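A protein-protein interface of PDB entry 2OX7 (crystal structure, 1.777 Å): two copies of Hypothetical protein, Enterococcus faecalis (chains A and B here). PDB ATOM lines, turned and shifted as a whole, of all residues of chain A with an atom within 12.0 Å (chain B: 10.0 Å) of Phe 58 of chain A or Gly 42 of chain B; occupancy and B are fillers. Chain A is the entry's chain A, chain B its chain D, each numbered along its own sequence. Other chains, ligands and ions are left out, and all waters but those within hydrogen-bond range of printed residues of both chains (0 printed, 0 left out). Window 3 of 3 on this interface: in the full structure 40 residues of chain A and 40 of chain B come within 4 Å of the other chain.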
ATOM      1  N   LEU A  24     -22.864  22.012   7.383  1.00  0.00           N
ATOM      2  CA  LEU A  24     -23.400  23.237   7.986  1.00  0.00           C
ATOM      3  C   LEU A  24     -24.734  23.595   7.342  1.00  0.00           C
ATOM      4  O   LEU A  24     -24.825  23.710   6.121  1.00  0.00           O
ATOM      5  CB  LEU A  24     -22.392  24.407   7.871  1.00  0.00           C
ATOM      6  CG  LEU A  24     -21.215  24.513   8.860  1.00  0.00           C
ATOM      7  CD1 LEU A  24     -20.355  23.273   8.918  1.00  0.00           C
ATOM      8  CD2 LEU A  24     -20.313  25.714   8.501  1.00  0.00           C
ATOM      9  N   ASP A  26     -28.447  25.977   7.280  1.00  0.00           N
ATOM     10  CA  ASP A  26     -29.126  27.167   7.761  1.00  0.00           C
ATOM     11  C   ASP A  26     -30.301  26.665   8.611  1.00  0.00           C
ATOM     12  O   ASP A  26     -30.381  25.470   8.916  1.00  0.00           O
ATOM     13  CB  ASP A  26     -29.540  28.067   6.594  1.00  0.00           C
ATOM     14  CG  ASP A  26     -30.801  27.613   5.938  1.00  0.00           C
ATOM     15  OD1 ASP A  26     -31.877  28.067   6.393  1.00  0.00           O
ATOM     16  OD2 ASP A  26     -30.725  26.812   4.975  1.00  0.00           O
ATOM     17  N   SER A  30     -31.407  23.534   4.825  1.00  0.00           N
ATOM     18  CA  SER A  30     -30.623  23.397   3.607  1.00  0.00           C
ATOM     19  C   SER A  30     -29.157  23.440   3.986  1.00  0.00           C
ATOM     20  O   SER A  30     -28.734  24.333   4.717  1.00  0.00           O
ATOM     21  CB  SER A  30     -30.937  24.519   2.620  1.00  0.00           C
ATOM     22  OG  SER A  30     -32.330  24.590   2.367  1.00  0.00           O
ATOM     23  N   MET A  31     -28.396  22.458   3.514  1.00  0.00           N
ATOM     24  CA  MET A  31     -26.952  22.490   3.698  1.00  0.00           C
ATOM     25  C   MET A  31     -26.353  23.568   2.805  1.00  0.00           C
ATOM     26  O   MET A  31     -26.532  23.546   1.580  1.00  0.00           O
ATOM     27  CB  MET A  31     -26.307  21.156   3.387  1.00  0.00           C
ATOM     28  CG  MET A  31     -24.848  21.124   3.741  1.00  0.00           C
ATOM     29  SD  MET A  31     -24.014  19.427   3.331  1.00  0.00           S
ATOM     30  CE  MET A  31     -24.724  19.101   1.539  1.00  0.00           C
ATOM     31  N   ILE A  32     -25.664  24.510   3.438  1.00  0.00           N
ATOM     32  CA  ILE A  32     -25.124  25.666   2.722  1.00  0.00           C
ATOM     33  C   ILE A  32     -23.596  25.702   2.752  1.00  0.00           C
ATOM     34  O   ILE A  32     -22.972  26.453   1.994  1.00  0.00           O
ATOM     35  CB  ILE A  32     -25.764  27.000   3.193  1.00  0.00           C
ATOM     36  CG1 ILE A  32     -25.510  27.249   4.691  1.00  0.00           C
ATOM     37  CG2 ILE A  32     -27.265  27.024   2.837  1.00  0.00           C
ATOM     38  CD1 ILE A  32     -25.848  28.692   5.168  1.00  0.00           C
ATOM     39  N   ALA A  33     -22.994  24.875   3.607  1.00  0.00           N
ATOM     40  CA  ALA A  33     -21.536  24.764   3.663  1.00  0.00           C
ATOM     41  C   ALA A  33     -21.099  23.389   4.123  1.00  0.00           C
ATOM     42  O   ALA A  33     -21.886  22.623   4.690  1.00  0.00           O
ATOM     43  CB  ALA A  33     -20.935  25.847   4.585  1.00  0.00           C
ATOM     44  N   ILE A  34     -19.831  23.096   3.881  1.00  0.00           N
ATOM     45  CA  ILE A  34     -19.220  21.900   4.409  1.00  0.00           C
ATOM     46  C   ILE A  34     -17.794  22.195   4.853  1.00  0.00           C
ATOM     47  O   ILE A  34     -17.010  22.810   4.116  1.00  0.00           O
ATOM     48  CB  ILE A  34     -19.322  20.719   3.393  1.00  0.00           C
ATOM     49  CG1 ILE A  34     -18.900  19.399   4.033  1.00  0.00           C
ATOM     50  CG2 ILE A  34     -18.565  21.011   2.087  1.00  0.00           C
ATOM     51  CD1 ILE A  34     -19.331  18.189   3.199  1.00  0.00           C
ATOM     52  N   TYR A  54     -12.841  23.404   2.972  1.00  0.00           N
ATOM     53  CA  TYR A  54     -14.258  23.703   3.052  1.00  0.00           C
ATOM     54  C   TYR A  54     -14.836  23.967   1.674  1.00  0.00           C
ATOM     55  O   TYR A  54     -14.102  24.059   0.676  1.00  0.00           O
ATOM     56  CB  TYR A  54     -14.500  24.913   3.969  1.00  0.00           C
ATOM     57  CG  TYR A  54     -14.153  26.255   3.333  1.00  0.00           C
ATOM     58  CD1 TYR A  54     -15.148  27.067   2.798  1.00  0.00           C
ATOM     59  CD2 TYR A  54     -12.828  26.697   3.256  1.00  0.00           C
ATOM     60  CE1 TYR A  54     -14.843  28.304   2.202  1.00  0.00           C
ATOM     61  CE2 TYR A  54     -12.509  27.940   2.657  1.00  0.00           C
ATOM     62  CZ  TYR A  54     -13.529  28.727   2.133  1.00  0.00           C
ATOM     63  OH  TYR A  54     -13.245  29.945   1.535  1.00  0.00           O
ATOM     64  N   ASP A  55     -16.157  24.100   1.624  1.00  0.00           N
ATOM     65  CA  ASP A  55     -16.846  24.582   0.438  1.00  0.00           C
ATOM     66  C   ASP A  55     -18.179  25.186   0.845  1.00  0.00           C
ATOM     67  O   ASP A  55     -18.723  24.838   1.895  1.00  0.00           O
ATOM     68  CB  ASP A  55     -17.063  23.457  -0.571  1.00  0.00           C
ATOM     69  CG  ASP A  55     -17.166  23.971  -1.997  1.00  0.00           C
ATOM     70  OD1 ASP A  55     -17.223  25.211  -2.176  1.00  0.00           O
ATOM     71  OD2 ASP A  55     -17.187  23.146  -2.945  1.00  0.00           O
ATOM     72  N   THR A  56     -18.705  26.100   0.041  1.00  0.00           N
ATOM     73  CA  THR A  56     -20.009  26.694   0.369  1.00  0.00           C
ATOM     74  C   THR A  56     -20.927  26.725  -0.842  1.00  0.00           C
ATOM     75  O   THR A  56     -20.483  26.513  -1.973  1.00  0.00           O
ATOM     76  CB  THR A  56     -19.922  28.111   1.045  1.00  0.00           C
ATOM     77  OG1 THR A  56     -20.042  29.145   0.050  1.00  0.00           O
ATOM     78  CG2 THR A  56     -18.632  28.295   1.854  1.00  0.00           C
ATOM     79  N   THR A  57     -22.206  26.982  -0.602  1.00  0.00           N
ATOM     80  CA  THR A  57     -23.208  26.919  -1.656  1.00  0.00           C
ATOM     81  C   THR A  57     -23.167  28.147  -2.575  1.00  0.00           C
ATOM     82  O   THR A  57     -23.804  28.158  -3.638  1.00  0.00           O
ATOM     83  CB  THR A  57     -24.622  26.745  -1.067  1.00  0.00           C
ATOM     84  OG1 THR A  57     -25.529  26.358  -2.108  1.00  0.00           O
ATOM     85  CG2 THR A  57     -25.103  28.031  -0.391  1.00  0.00           C
ATOM     86  N   PHE A  58     -22.430  29.172  -2.138  1.00  0.00           N
ATOM     87  CA  PHE A  58     -22.187  30.388  -2.920  1.00  0.00           C
ATOM     88  C   PHE A  58     -21.668  30.013  -4.305  1.00  0.00           C
ATOM     89  O   PHE A  58     -22.169  30.504  -5.320  1.00  0.00           O
ATOM     90  CB  PHE A  58     -21.153  31.268  -2.208  1.00  0.00           C
ATOM     91  CG  PHE A  58     -21.434  32.755  -2.294  1.00  0.00           C
ATOM     92  CD1 PHE A  58     -21.866  33.457  -1.168  1.00  0.00           C
ATOM     93  CD2 PHE A  58     -21.257  33.451  -3.491  1.00  0.00           C
ATOM     94  CE1 PHE A  58     -22.129  34.825  -1.231  1.00  0.00           C
ATOM     95  CE2 PHE A  58     -21.521  34.813  -3.568  1.00  0.00           C
ATOM     96  CZ  PHE A  58     -21.954  35.504  -2.433  1.00  0.00           C
ATOM     97  N   ASN A  59     -20.698  29.093  -4.329  1.00  0.00           N
ATOM     98  CA  ASN A  59     -19.960  28.726  -5.538  1.00  0.00           C
ATOM     99  C   ASN A  59     -20.722  27.805  -6.491  1.00  0.00           C
ATOM    100  O   ASN A  59     -20.161  27.349  -7.498  1.00  0.00           O
ATOM    101  CB  ASN A  59     -18.637  28.049  -5.160  1.00  0.00           C
ATOM    102  CG  ASN A  59     -17.939  28.727  -4.002  1.00  0.00           C
ATOM    103  OD1 ASN A  59     -17.304  29.773  -4.160  1.00  0.00           O
ATOM    104  ND2 ASN A  59     -18.044  28.125  -2.825  1.00  0.00           N
ATOM    105  N   TRP A  60     -21.990  27.536  -6.185  1.00  0.00           N
ATOM    106  CA  TRP A  60     -22.717  26.472  -6.868  1.00  0.00           C
ATOM    107  C   TRP A  60     -24.176  26.792  -7.118  1.00  0.00           C
ATOM    108  O   TRP A  60     -24.859  27.362  -6.265  1.00  0.00           O
ATOM    109  CB  TRP A  60     -22.634  25.182  -6.045  1.00  0.00           C
ATOM    110  CG  TRP A  60     -21.247  24.645  -5.911  1.00  0.00           C
ATOM    111  CD1 TRP A  60     -20.371  24.881  -4.894  1.00  0.00           C
ATOM    112  CD2 TRP A  60     -20.574  23.775  -6.830  1.00  0.00           C
ATOM    113  NE1 TRP A  60     -19.190  24.215  -5.120  1.00  0.00           N
ATOM    114  CE2 TRP A  60     -19.288  23.525  -6.301  1.00  0.00           C
ATOM    115  CE3 TRP A  60     -20.935  23.177  -8.047  1.00  0.00           C
ATOM    116  CZ2 TRP A  60     -18.353  22.698  -6.948  1.00  0.00           C
ATOM    117  CZ3 TRP A  60     -19.999  22.351  -8.695  1.00  0.00           C
ATOM    118  CH2 TRP A  60     -18.726  22.123  -8.140  1.00  0.00           C
ATOM    119  N   ASP A  61     -24.649  26.396  -8.292  1.00  0.00           N
ATOM    120  CA  ASP A  61     -26.068  26.445  -8.600  1.00  0.00           C
ATOM    121  C   ASP A  61     -26.781  25.427  -7.711  1.00  0.00           C
ATOM    122  O   ASP A  61     -27.777  25.756  -7.048  1.00  0.00           O
ATOM    123  CB  ASP A  61     -26.295  26.150 -10.082  1.00  0.00           C
ATOM    124  CG  ASP A  61     -25.441  27.029 -10.991  1.00  0.00           C
ATOM    125  OD1 ASP A  61     -24.195  26.861 -10.991  1.00  0.00           O
ATOM    126  OD2 ASP A  61     -26.015  27.883 -11.704  1.00  0.00           O
ATOM    127  N   GLU A  62     -26.258  24.200  -7.692  1.00  0.00           N
ATOM    128  CA  GLU A  62     -26.688  23.178  -6.739  1.00  0.00           C
ATOM    129  C   GLU A  62     -25.458  22.616  -6.038  1.00  0.00           C
ATOM    130  O   GLU A  62     -24.530  22.102  -6.685  1.00  0.00           O
ATOM    131  CB  GLU A  62     -27.561  22.091  -7.408  1.00  0.00           C
ATOM    132  CG  GLU A  62     -26.931  20.703  -7.591  1.00  0.00           C
ATOM    133  CD  GLU A  62     -26.212  20.524  -8.928  1.00  0.00           C
ATOM    134  OE1 GLU A  62     -25.006  20.174  -8.922  1.00  0.00           O
ATOM    135  OE2 GLU A  62     -26.858  20.717  -9.987  1.00  0.00           O
ATOM    136  N   PHE A  63     -25.443  22.763  -4.715  1.00  0.00           N
ATOM    137  CA  PHE A  63     -24.341  22.318  -3.876  1.00  0.00           C
ATOM    138  C   PHE A  63     -24.162  20.813  -4.083  1.00  0.00           C
ATOM    139  O   PHE A  63     -25.076  20.046  -3.803  1.00  0.00           O
ATOM    140  CB  PHE A  63     -24.654  22.661  -2.423  1.00  0.00           C
ATOM    141  CG  PHE A  63     -23.451  22.698  -1.527  1.00  0.00           C
ATOM    142  CD1 PHE A  63     -22.296  23.380  -1.901  1.00  0.00           C
ATOM    143  CD2 PHE A  63     -23.477  22.051  -0.292  1.00  0.00           C
ATOM    144  CE1 PHE A  63     -21.183  23.417  -1.056  1.00  0.00           C
ATOM    145  CE2 PHE A  63     -22.373  22.086   0.554  1.00  0.00           C
ATOM    146  CZ  PHE A  63     -21.227  22.776   0.177  1.00  0.00           C
ATOM    147  N   PRO A  64     -23.001  20.392  -4.619  1.00  0.00           N
ATOM    148  CA  PRO A  64     -22.862  19.023  -5.135  1.00  0.00           C
ATOM    149  C   PRO A  64     -22.407  18.000  -4.087  1.00  0.00           C
ATOM    150  O   PRO A  64     -21.618  17.114  -4.395  1.00  0.00           O
ATOM    151  CB  PRO A  64     -21.769  19.189  -6.184  1.00  0.00           C
ATOM    152  CG  PRO A  64     -20.858  20.198  -5.577  1.00  0.00           C
ATOM    153  CD  PRO A  64     -21.747  21.154  -4.800  1.00  0.00           C
ATOM    154  N   TYR A  65     -22.884  18.133  -2.861  1.00  0.00           N
ATOM    155  CA  TYR A  65     -22.469  17.230  -1.784  1.00  0.00           C
ATOM    156  C   TYR A  65     -23.689  16.541  -1.204  1.00  0.00           C
ATOM    157  O   TYR A  65     -24.716  17.188  -0.969  1.00  0.00           O
ATOM    158  CB  TYR A  65     -21.728  17.991  -0.694  1.00  0.00           C
ATOM    159  CG  TYR A  65     -20.466  18.671  -1.181  1.00  0.00           C
ATOM    160  CD1 TYR A  65     -19.242  18.017  -1.164  1.00  0.00           C
ATOM    161  CD2 TYR A  65     -20.507  19.982  -1.673  1.00  0.00           C
ATOM    162  CE1 TYR A  65     -18.087  18.647  -1.613  1.00  0.00           C
ATOM    163  CE2 TYR A  65     -19.364  20.618  -2.120  1.00  0.00           C
ATOM    164  CZ  TYR A  65     -18.159  19.951  -2.094  1.00  0.00           C
ATOM    165  OH  TYR A  65     -17.014  20.600  -2.533  1.00  0.00           O
ATOM    166  N   GLN B  39     -22.242  32.782   9.003  1.00  0.00           N
ATOM    167  CA  GLN B  39     -22.783  33.238   7.734  1.00  0.00           C
ATOM    168  C   GLN B  39     -21.882  32.790   6.599  1.00  0.00           C
ATOM    169  O   GLN B  39     -20.692  32.537   6.803  1.00  0.00           O
ATOM    170  CB  GLN B  39     -22.849  34.757   7.701  1.00  0.00           C
ATOM    171  CG  GLN B  39     -23.864  35.399   8.610  1.00  0.00           C
ATOM    172  CD  GLN B  39     -23.706  36.909   8.631  1.00  0.00           C
ATOM    173  OE1 GLN B  39     -24.390  37.602   9.385  1.00  0.00           O
ATOM    174  NE2 GLN B  39     -22.793  37.426   7.804  1.00  0.00           N
ATOM    175  N   ILE B  40     -22.457  32.702   5.404  1.00  0.00           N
ATOM    176  CA  ILE B  40     -21.682  32.505   4.187  1.00  0.00           C
ATOM    177  C   ILE B  40     -21.570  33.859   3.487  1.00  0.00           C
ATOM    178  O   ILE B  40     -22.558  34.409   2.982  1.00  0.00           O
ATOM    179  CB  ILE B  40     -22.297  31.406   3.264  1.00  0.00           C
ATOM    180  CG1 ILE B  40     -21.807  30.007   3.665  1.00  0.00           C
ATOM    181  CG2 ILE B  40     -21.889  31.598   1.821  1.00  0.00           C
ATOM    182  CD1 ILE B  40     -22.105  29.590   5.072  1.00  0.00           C
ATOM    183  N   LYS B  41     -20.359  34.406   3.499  1.00  0.00           N
ATOM    184  CA  LYS B  41     -20.080  35.667   2.830  1.00  0.00           C
ATOM    185  C   LYS B  41     -18.896  35.470   1.900  1.00  0.00           C
ATOM    186  O   LYS B  41     -17.741  35.648   2.299  1.00  0.00           O
ATOM    187  CB  LYS B  41     -19.798  36.786   3.844  1.00  0.00           C
ATOM    188  CG  LYS B  41     -20.569  38.098   3.599  1.00  0.00           C
ATOM    189  CD  LYS B  41     -20.528  38.562   2.133  1.00  0.00           C
ATOM    190  CE  LYS B  41     -20.980  40.020   1.983  1.00  0.00           C
ATOM    191  NZ  LYS B  41     -22.412  40.258   2.353  1.00  0.00           N
ATOM    192  N   GLY B  42     -19.201  35.060   0.671  1.00  0.00           N
ATOM    193  CA  GLY B  42     -18.216  34.997  -0.406  1.00  0.00           C
ATOM    194  C   GLY B  42     -18.456  36.090  -1.425  1.00  0.00           C
ATOM    195  O   GLY B  42     -19.330  36.946  -1.228  1.00  0.00           O
ATOM    196  N   SER B  43     -17.691  36.063  -2.518  1.00  0.00           N
ATOM    197  CA  SER B  43     -17.756  37.135  -3.510  1.00  0.00           C
ATOM    198  C   SER B  43     -17.014  36.825  -4.828  1.00  0.00           C
ATOM    199  O   SER B  43     -15.834  37.166  -4.970  1.00  0.00           O
ATOM    200  CB  SER B  43     -17.208  38.437  -2.892  1.00  0.00           C
ATOM    201  OG  SER B  43     -18.067  39.540  -3.130  1.00  0.00           O
ATOM    202  N   PRO B  44     -17.670  36.121  -5.775  1.00  0.00           N
ATOM    203  CA  PRO B  44     -18.764  35.147  -5.686  1.00  0.00           C
ATOM    204  C   PRO B  44     -18.262  33.708  -5.924  1.00  0.00           C
ATOM    205  O   PRO B  44     -18.941  32.737  -5.566  1.00  0.00           O
ATOM    206  CB  PRO B  44     -19.681  35.573  -6.836  1.00  0.00           C
ATOM    207  CG  PRO B  44     -18.732  36.269  -7.863  1.00  0.00           C
ATOM    208  CD  PRO B  44     -17.370  36.427  -7.188  1.00  0.00           C
ATOM    209  N   GLY B  45     -17.092  33.593  -6.555  1.00  0.00           N
ATOM    210  CA  GLY B  45     -16.420  32.311  -6.791  1.00  0.00           C
ATOM    211  C   GLY B  45     -15.310  32.099  -5.778  1.00  0.00           C
ATOM    212  O   GLY B  45     -14.501  31.171  -5.906  1.00  0.00           O
ATOM    213  N   THR B  46     -15.270  32.985  -4.780  1.00  0.00           N
ATOM    214  CA  THR B  46     -14.401  32.846  -3.618  1.00  0.00           C
ATOM    215  C   THR B  46     -15.227  33.153  -2.362  1.00  0.00           C
ATOM    216  O   THR B  46     -15.181  34.268  -1.810  1.00  0.00           O
ATOM    217  CB  THR B  46     -13.173  33.778  -3.687  1.00  0.00           C
ATOM    218  OG1 THR B  46     -13.609  35.114  -3.970  1.00  0.00           O
ATOM    219  CG2 THR B  46     -12.181  33.312  -4.759  1.00  0.00           C
ATOM    220  N   SER B  47     -15.999  32.160  -1.932  1.00  0.00           N
ATOM    221  CA  SER B  47     -16.812  32.285  -0.729  1.00  0.00           C
ATOM    222  C   SER B  47     -16.052  31.892   0.528  1.00  0.00           C
ATOM    223  O   SER B  47     -14.996  31.255   0.463  1.00  0.00           O
ATOM    224  CB  SER B  47     -18.087  31.463  -0.855  1.00  0.00           C
ATOM    225  OG  SER B  47     -17.803  30.208  -1.438  1.00  0.00           O
ATOM    226  N   GLU B  48     -16.610  32.280   1.669  1.00  0.00           N
ATOM    227  CA  GLU B  48     -15.995  32.049   2.966  1.00  0.00           C
ATOM    228  C   GLU B  48     -17.083  31.693   3.989  1.00  0.00           C
ATOM    229  O   GLU B  48     -18.242  32.090   3.833  1.00  0.00           O
ATOM    230  CB  GLU B  48     -15.229  33.314   3.384  1.00  0.00           C
ATOM    231  CG  GLU B  48     -14.488  33.229   4.712  1.00  0.00           C
ATOM    232  CD  GLU B  48     -13.757  34.521   5.058  1.00  0.00           C
ATOM    233  OE1 GLU B  48     -12.616  34.704   4.573  1.00  0.00           O
ATOM    234  OE2 GLU B  48     -14.318  35.354   5.819  1.00  0.00           O
ATOM    235  N   ILE B  49     -16.717  30.923   5.015  1.00  0.00           N
ATOM    236  CA  ILE B  49     -17.617  30.677   6.145  1.00  0.00           C
ATOM    237  C   ILE B  49     -17.216  31.643   7.235  1.00  0.00           C
ATOM    238  O   ILE B  49     -16.130  31.523   7.795  1.00  0.00           O
ATOM    239  CB  ILE B  49     -17.516  29.225   6.716  1.00  0.00           C
ATOM    240  CG1 ILE B  49     -17.816  28.174   5.642  1.00  0.00           C
ATOM    241  CG2 ILE B  49     -18.457  29.043   7.911  1.00  0.00           C
ATOM    242  CD1 ILE B  49     -17.375  26.771   6.031  1.00  0.00           C
ATOM    243  N   GLU B  50     -18.073  32.616   7.526  1.00  0.00           N
ATOM    244  CA  GLU B  50     -17.778  33.536   8.616  1.00  0.00           C
ATOM    245  C   GLU B  50     -18.440  33.019   9.874  1.00  0.00           C
ATOM    246  O   GLU B  50     -19.655  33.130  10.038  1.00  0.00           O
ATOM    247  CB  GLU B  50     -18.226  34.981   8.330  1.00  0.00           C
ATOM    248  CG  GLU B  50     -17.772  35.963   9.431  1.00  0.00           C
ATOM    249  CD  GLU B  50     -18.712  37.148   9.647  1.00  0.00           C
ATOM    250  OE1 GLU B  50     -18.611  38.133   8.881  1.00  0.00           O
ATOM    251  OE2 GLU B  50     -19.531  37.108  10.602  1.00  0.00           O
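Of the printed residues of chain A, Gly 42 of chain B touches Phe 58 (3.2 Å).
Of chain B, only Pro 44, Gly 45, Thr 46 and Ser 47 come within 4 Å of Asn 59 of chain A.
Ile 40 of chain B touches just these residues of chain A: Ile 32 (3.9 Å), Ala 33 (3.95 Å), Thr 56 (3.5 Å) and Phe 58 (3.5 Å).
No residue of chain A comes within 4 Å of Lys 41 of chain B.
Of the printed residues of chain A, Pro 44 of chain B touches Phe 58 (3.2 Å) and Asn 59 (3.7 Å).
Gly 45 of chain B touches one residue of chain A.
Thr 46 of chain B touches just one residue of chain A: Asn 59.
Glu 48 of chain B touches one residue of chain A.
Printed residues of chain B within 4 Å of Leu 24 of chain A: Ile 49 (3.9 Å).
Of the printed residues of chain B, Ala 33 of chain A touches Ile 40 (3.95 Å) and Ile 49 (3.95 Å).
Of the printed residues of chain A, Ile 49 of chain B touches Leu 24 (3.9 Å), Ala 33 (3.95 Å), Tyr 54 (3.9 Å) and Thr 56 (3.9 Å).
The nearest residue of chain B that does not touch Phe 58 of chain A is Ser 43 of chain B (4.2 Å).
The nearest printed residue of chain A that does not touch Ile 49 of chain B is Ile 34 of chain A (4.4 Å).
Among the printed residues, merely in contact across the chains: Leu 24 of chain A with Ile 49 of chain B (3.9 Å), Ile 32 of chain A with Ile 40 of chain B (3.9 Å), Ala 33 of chain A with Ile 40 of chain B (3.95 Å), Ala 33 of chain A with Ile 49 of chain B (3.95 Å), Tyr 54 of chain A with Glu 48 of chain B (3.7 Å), Tyr 54 of chain A with Ile 49 of chain B (3.9 Å), Thr 56 of chain A with Ile 40 of chain B (3.5 Å), Thr 56 of chain A with Ile 49 of chain B (3.9 Å), Phe 58 of chain A with Ile 40 of chain B (3.5 Å), Phe 58 of chain A with Gly 42 of chain B (3.2 Å), Phe 58 of chain A with Pro 44 of chain B (3.2 Å), Phe 58 of chain A with Ser 47 of chain B (3.4 Å), Asn 59 of chain A with Pro 44 of chain B (3.7 Å), Asn 59 of chain A with Gly 45 of chain B (3.5 Å) and Asn 59 of chain A with Thr 46 of chain B (3.9 Å).
Of the 12 printed residues of chain B, 8 touch a printed residue of chain A.
Printed residues of chain B that touch a printed residue of chain A: Ile 40, Gly 42, Pro 44, Gly 45, Thr 46, Ser 47, Glu 48 and Ile 49.
Hydrophobic or aromatic side chains of chain B within 4 Å of the printed part of chain A: Ile 40, Pro 44 and Ile 49.
Hydrophobic or aromatic side chains of chain A that line the printed part of chain B: Leu 24, Ile 32, Ala 33, Tyr 54 and Phe 58.
Among the printed residues, 18 pairs touch across the chains.
The backbone carbonyl oxygen (O) of Ile 32 of chain A lies within hydrogen-bond range of the backbone NH (N) of Thr 57 of chain A (2.8 Å).
The side-chain carboxylate (OD1) of Asp 55 of chain A sits at hydrogen-bond distance from the side-chain amide nitrogen (ND2) of Asn 59 of chain A (3.1 Å).
OG1 of Thr 56 of chain A lies close to N of Phe 58 of chain A.
O of Thr 56 of chain A is in hydrogen-bond range of ND2 of Asn 59 of chain A.
N of Leu 24 of chain A lies within hydrogen-bond range of O of Ala 33 of chain A (2.9 Å).
N of Ile 32 of chain A is in hydrogen-bond range of O of Leu 24 of chain A (2.9 Å).
No position is printed for both chains.
Of the 18 pairs that touch across the chains among the printed residues, none has its exchanged pair printed and touching as well.
The side-chain hydroxyl of Ser 47 of chain B is in hydrogen-bond range of the side-chain hydroxyl of Thr 56 of chain A, 2.9 Å away.
The side-chain hydroxyl (OG) of Ser 47 of chain B sits at hydrogen-bond distance from the side-chain amide nitrogen (ND2) of Asn 59 of chain A.
The backbone carbonyl oxygen of Ser 47 of chain B sits at hydrogen-bond distance from the side-chain hydroxyl of Tyr 54 of chain A, 2.4 Å away.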
